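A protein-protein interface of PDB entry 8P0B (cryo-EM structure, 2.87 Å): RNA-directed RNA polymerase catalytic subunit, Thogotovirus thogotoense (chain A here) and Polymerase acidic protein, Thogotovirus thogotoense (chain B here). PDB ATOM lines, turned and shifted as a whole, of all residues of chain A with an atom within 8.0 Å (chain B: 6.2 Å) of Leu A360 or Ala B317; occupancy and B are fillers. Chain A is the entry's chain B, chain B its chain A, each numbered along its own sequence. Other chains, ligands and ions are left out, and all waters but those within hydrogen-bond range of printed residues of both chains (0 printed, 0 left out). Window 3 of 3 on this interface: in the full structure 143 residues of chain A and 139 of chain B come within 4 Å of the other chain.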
ATOM      1  N   VAL A 354     -11.196  36.941   1.126  1.00  0.00           N
ATOM      2  CA  VAL A 354     -11.821  35.873   0.355  1.00  0.00           C
ATOM      3  C   VAL A 354     -11.276  34.527   0.810  1.00  0.00           C
ATOM      4  O   VAL A 354     -10.073  34.370   1.049  1.00  0.00           O
ATOM      5  CB  VAL A 354     -11.594  36.089  -1.152  1.00  0.00           C
ATOM      6  CG1 VAL A 354     -12.412  37.268  -1.644  1.00  0.00           C
ATOM      7  CG2 VAL A 354     -10.119  36.309  -1.453  1.00  0.00           C
ATOM      8  N   TYR A 355     -12.169  33.548   0.932  1.00  0.00           N
ATOM      9  CA  TYR A 355     -11.812  32.187   1.295  1.00  0.00           C
ATOM     10  C   TYR A 355     -12.540  31.225   0.370  1.00  0.00           C
ATOM     11  O   TYR A 355     -13.614  31.538  -0.153  1.00  0.00           O
ATOM     12  CB  TYR A 355     -12.174  31.878   2.755  1.00  0.00           C
ATOM     13  CG  TYR A 355     -11.276  32.549   3.769  1.00  0.00           C
ATOM     14  CD1 TYR A 355     -11.388  33.906   4.037  1.00  0.00           C
ATOM     15  CD2 TYR A 355     -10.319  31.823   4.464  1.00  0.00           C
ATOM     16  CE1 TYR A 355     -10.571  34.521   4.962  1.00  0.00           C
ATOM     17  CE2 TYR A 355      -9.497  32.428   5.392  1.00  0.00           C
ATOM     18  CZ  TYR A 355      -9.627  33.779   5.637  1.00  0.00           C
ATOM     19  OH  TYR A 355      -8.810  34.386   6.561  1.00  0.00           O
ATOM     20  N   THR A 356     -11.946  30.050   0.171  1.00  0.00           N
ATOM     21  CA  THR A 356     -12.502  29.026  -0.702  1.00  0.00           C
ATOM     22  C   THR A 356     -12.569  27.705   0.048  1.00  0.00           C
ATOM     23  O   THR A 356     -11.594  27.302   0.690  1.00  0.00           O
ATOM     24  CB  THR A 356     -11.662  28.863  -1.973  1.00  0.00           C
ATOM     25  OG1 THR A 356     -10.279  28.733  -1.621  1.00  0.00           O
ATOM     26  CG2 THR A 356     -11.838  30.065  -2.887  1.00  0.00           C
ATOM     27  N   LYS A 357     -13.717  27.038  -0.037  1.00  0.00           N
ATOM     28  CA  LYS A 357     -13.945  25.732   0.579  1.00  0.00           C
ATOM     29  C   LYS A 357     -14.308  24.771  -0.547  1.00  0.00           C
ATOM     30  O   LYS A 357     -15.486  24.545  -0.831  1.00  0.00           O
ATOM     31  CB  LYS A 357     -15.047  25.816   1.638  1.00  0.00           C
ATOM     32  CG  LYS A 357     -15.482  24.484   2.233  1.00  0.00           C
ATOM     33  CD  LYS A 357     -16.795  24.632   2.991  1.00  0.00           C
ATOM     34  CE  LYS A 357     -16.638  24.307   4.466  1.00  0.00           C
ATOM     35  NZ  LYS A 357     -17.793  24.796   5.270  1.00  0.00           N
ATOM     36  N   GLY A 358     -13.290  24.203  -1.188  1.00  0.00           N
ATOM     37  CA  GLY A 358     -13.516  23.360  -2.344  1.00  0.00           C
ATOM     38  C   GLY A 358     -13.585  24.174  -3.617  1.00  0.00           C
ATOM     39  O   GLY A 358     -12.553  24.535  -4.190  1.00  0.00           O
ATOM     40  N   LYS A 359     -14.804  24.469  -4.072  1.00  0.00           N
ATOM     41  CA  LYS A 359     -15.023  25.288  -5.258  1.00  0.00           C
ATOM     42  C   LYS A 359     -15.893  26.505  -4.970  1.00  0.00           C
ATOM     43  O   LYS A 359     -16.325  27.180  -5.912  1.00  0.00           O
ATOM     44  CB  LYS A 359     -15.654  24.446  -6.371  1.00  0.00           C
ATOM     45  CG  LYS A 359     -14.703  23.431  -6.987  1.00  0.00           C
ATOM     46  CD  LYS A 359     -15.382  22.614  -8.073  1.00  0.00           C
ATOM     47  CE  LYS A 359     -14.454  21.541  -8.623  1.00  0.00           C
ATOM     48  NZ  LYS A 359     -15.135  20.658  -9.613  1.00  0.00           N
ATOM     49  N   LEU A 360     -16.156  26.808  -3.701  1.00  0.00           N
ATOM     50  CA  LEU A 360     -16.991  27.939  -3.330  1.00  0.00           C
ATOM     51  C   LEU A 360     -16.130  29.191  -3.187  1.00  0.00           C
ATOM     52  O   LEU A 360     -14.949  29.209  -3.544  1.00  0.00           O
ATOM     53  CB  LEU A 360     -17.746  27.644  -2.035  1.00  0.00           C
ATOM     54  CG  LEU A 360     -18.180  26.202  -1.778  1.00  0.00           C
ATOM     55  CD1 LEU A 360     -19.017  26.128  -0.512  1.00  0.00           C
ATOM     56  CD2 LEU A 360     -18.955  25.647  -2.957  1.00  0.00           C
ATOM     57  N   THR A 361     -16.724  30.259  -2.658  1.00  0.00           N
ATOM     58  CA  THR A 361     -15.997  31.490  -2.376  1.00  0.00           C
ATOM     59  C   THR A 361     -16.849  32.328  -1.435  1.00  0.00           C
ATOM     60  O   THR A 361     -18.026  32.568  -1.718  1.00  0.00           O
ATOM     61  CB  THR A 361     -15.687  32.264  -3.664  1.00  0.00           C
ATOM     62  OG1 THR A 361     -14.481  31.759  -4.249  1.00  0.00           O
ATOM     63  CG2 THR A 361     -15.521  33.753  -3.382  1.00  0.00           C
ATOM     64  N   ASP A 362     -16.260  32.764  -0.324  1.00  0.00           N
ATOM     65  CA  ASP A 362     -16.980  33.548   0.668  1.00  0.00           C
ATOM     66  C   ASP A 362     -16.061  34.607   1.254  1.00  0.00           C
ATOM     67  O   ASP A 362     -14.877  34.355   1.484  1.00  0.00           O
ATOM     68  CB  ASP A 362     -17.526  32.660   1.793  1.00  0.00           C
ATOM     69  CG  ASP A 362     -18.316  33.444   2.821  1.00  0.00           C
ATOM     70  OD1 ASP A 362     -18.856  34.513   2.469  1.00  0.00           O
ATOM     71  OD2 ASP A 362     -18.395  32.992   3.982  1.00  0.00           O
ATOM     72  N   LYS B 310     -22.781  28.025  -9.490  1.00  0.00           N
ATOM     73  CA  LYS B 310     -23.003  28.031  -8.048  1.00  0.00           C
ATOM     74  C   LYS B 310     -23.363  26.636  -7.553  1.00  0.00           C
ATOM     75  O   LYS B 310     -22.834  26.167  -6.540  1.00  0.00           O
ATOM     76  CB  LYS B 310     -24.102  29.033  -7.696  1.00  0.00           C
ATOM     77  CG  LYS B 310     -24.724  28.829  -6.324  1.00  0.00           C
ATOM     78  CD  LYS B 310     -25.246  30.137  -5.741  1.00  0.00           C
ATOM     79  CE  LYS B 310     -26.200  30.842  -6.696  1.00  0.00           C
ATOM     80  NZ  LYS B 310     -26.834  32.037  -6.073  1.00  0.00           N
ATOM     81  N   ALA B 313     -20.433  24.190  -7.819  1.00  0.00           N
ATOM     82  CA  ALA B 313     -19.463  24.421  -6.757  1.00  0.00           C
ATOM     83  C   ALA B 313     -19.981  23.931  -5.410  1.00  0.00           C
ATOM     84  O   ALA B 313     -19.249  23.274  -4.662  1.00  0.00           O
ATOM     85  CB  ALA B 313     -19.116  25.910  -6.682  1.00  0.00           C
ATOM     86  N   SER B 314     -21.241  24.238  -5.089  1.00  0.00           N
ATOM     87  CA  SER B 314     -21.822  23.767  -3.837  1.00  0.00           C
ATOM     88  C   SER B 314     -21.840  22.248  -3.773  1.00  0.00           C
ATOM     89  O   SER B 314     -21.823  21.672  -2.680  1.00  0.00           O
ATOM     90  CB  SER B 314     -23.236  24.323  -3.672  1.00  0.00           C
ATOM     91  OG  SER B 314     -23.903  23.702  -2.588  1.00  0.00           O
ATOM     92  N   SER B 315     -21.872  21.582  -4.930  1.00  0.00           N
ATOM     93  CA  SER B 315     -21.814  20.127  -4.947  1.00  0.00           C
ATOM     94  C   SER B 315     -20.538  19.598  -4.307  1.00  0.00           C
ATOM     95  O   SER B 315     -20.508  18.438  -3.880  1.00  0.00           O
ATOM     96  CB  SER B 315     -21.925  19.614  -6.383  1.00  0.00           C
ATOM     97  OG  SER B 315     -22.822  20.406  -7.140  1.00  0.00           O
ATOM     98  N   SER B 316     -19.488  20.414  -4.235  1.00  0.00           N
ATOM     99  CA  SER B 316     -18.217  20.037  -3.625  1.00  0.00           C
ATOM    100  C   SER B 316     -17.947  20.850  -2.361  1.00  0.00           C
ATOM    101  O   SER B 316     -16.808  21.225  -2.073  1.00  0.00           O
ATOM    102  CB  SER B 316     -17.072  20.205  -4.620  1.00  0.00           C
ATOM    103  OG  SER B 316     -17.212  19.315  -5.713  1.00  0.00           O
ATOM    104  N   ALA B 317     -18.999  21.129  -1.589  1.00  0.00           N
ATOM    105  CA  ALA B 317     -18.857  21.936  -0.384  1.00  0.00           C
ATOM    106  C   ALA B 317     -18.199  21.181   0.764  1.00  0.00           C
ATOM    107  O   ALA B 317     -17.861  21.805   1.775  1.00  0.00           O
ATOM    108  CB  ALA B 317     -20.226  22.453   0.060  1.00  0.00           C
ATOM    109  N   SER B 318     -18.011  19.871   0.639  1.00  0.00           N
ATOM    110  CA  SER B 318     -17.379  19.079   1.693  1.00  0.00           C
ATOM    111  C   SER B 318     -15.892  19.404   1.724  1.00  0.00           C
ATOM    112  O   SER B 318     -15.115  18.910   0.904  1.00  0.00           O
ATOM    113  CB  SER B 318     -17.618  17.592   1.454  1.00  0.00           C
ATOM    114  OG  SER B 318     -16.846  16.801   2.342  1.00  0.00           O
ATOM    115  N   GLY B 319     -15.489  20.235   2.675  1.00  0.00           N
ATOM    116  CA  GLY B 319     -14.099  20.631   2.767  1.00  0.00           C
ATOM    117  C   GLY B 319     -13.895  21.615   3.895  1.00  0.00           C
ATOM    118  O   GLY B 319     -14.743  21.753   4.779  1.00  0.00           O
ATOM    119  N   GLU B 320     -12.752  22.298   3.857  1.00  0.00           N
ATOM    120  CA  GLU B 320     -12.387  23.277   4.870  1.00  0.00           C
ATOM    121  C   GLU B 320     -12.081  24.612   4.209  1.00  0.00           C
ATOM    122  O   GLU B 320     -11.444  24.660   3.152  1.00  0.00           O
ATOM    123  CB  GLU B 320     -11.176  22.809   5.682  1.00  0.00           C
ATOM    124  CG  GLU B 320     -10.542  23.904   6.527  1.00  0.00           C
ATOM    125  CD  GLU B 320      -9.706  23.358   7.668  1.00  0.00           C
ATOM    126  OE1 GLU B 320      -9.794  22.145   7.951  1.00  0.00           O
ATOM    127  OE2 GLU B 320      -8.961  24.147   8.285  1.00  0.00           O
ATOM    128  N   TRP B 321     -12.535  25.694   4.838  1.00  0.00           N
ATOM    129  CA  TRP B 321     -12.246  27.029   4.334  1.00  0.00           C
ATOM    130  C   TRP B 321     -10.745  27.283   4.348  1.00  0.00           C
ATOM    131  O   TRP B 321     -10.059  26.968   5.324  1.00  0.00           O
ATOM    132  CB  TRP B 321     -12.964  28.082   5.179  1.00  0.00           C
ATOM    133  CG  TRP B 321     -14.415  28.244   4.848  1.00  0.00           C
ATOM    134  CD1 TRP B 321     -15.477  27.981   5.664  1.00  0.00           C
ATOM    135  CD2 TRP B 321     -14.966  28.717   3.614  1.00  0.00           C
ATOM    136  NE1 TRP B 321     -16.653  28.255   5.013  1.00  0.00           N
ATOM    137  CE2 TRP B 321     -16.368  28.706   3.752  1.00  0.00           C
ATOM    138  CE3 TRP B 321     -14.411  29.143   2.405  1.00  0.00           C
ATOM    139  CZ2 TRP B 321     -17.220  29.109   2.727  1.00  0.00           C
ATOM    140  CZ3 TRP B 321     -15.261  29.539   1.388  1.00  0.00           C
ATOM    141  CH2 TRP B 321     -16.648  29.519   1.555  1.00  0.00           C
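Hydrophobic or aromatic side chains of chain B within 4 Å of the printed part of chain A: Ala B313, Ala B317 and Trp B321. Of the 9 printed residues of chain A, 7 touch a printed residue of chain B. Among the printed residues, no Asp or Glu carboxylate lies within 4 Å of a Lys or Arg side-chain nitrogen of the other chain.
Thr A356 touches Glu B320. O of Ser B316 touches O of Lys A357, 3.8 Å away. Lys A357 touches Ala B317. CE of Lys A357 touches O of Gly B319 (3.2 Å). Lys A357 touches Glu B320. Lys A357 touches Trp B321. O of Ser B316 touches CA of Gly A358, at 3.9 Å. CB of Ala B313 touches O of Lys A359, 3.2 Å away. Ala B313 touches Leu A360. Asp A362 touches Trp B321.
The backbone carbonyl oxygen (O) of Asp A362 sits at hydrogen-bond distance from the backbone NH (N) of Tyr A355.
Printed residues of chain B within 4 Å of Lys A357: Ser B316, Ala B317, Gly B319, Glu B320 and Trp B321. Of the printed residues of chain B, Lys A359 touches Ala B313. Leu A360 touches three residues of chain B. Thr A361 touches none of the printed residues of chain B. Of the printed residues of chain B, Asp A362 touches Trp B321. Printed residues of chain A within 4 Å of Ala B313: Lys A359 (3.2 Å) and Leu A360 (2.9 Å). Of the printed residues of chain A, Ser B314 touches Leu A360 (3.4 Å). Ser B315 touches none of the printed residues of chain A. Of the printed residues of chain A, Ala B317 touches Lys A357 and Leu A360. The nearest residue of chain B that does not touch Leu A360 is Trp B321 (4.2 Å). The nearest residue of chain A that does not touch Ala B317 is Gly A358 (5.9 Å). The nearest printed residue of chain A that does not touch Trp B321 is Thr A361 (4.1 Å).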
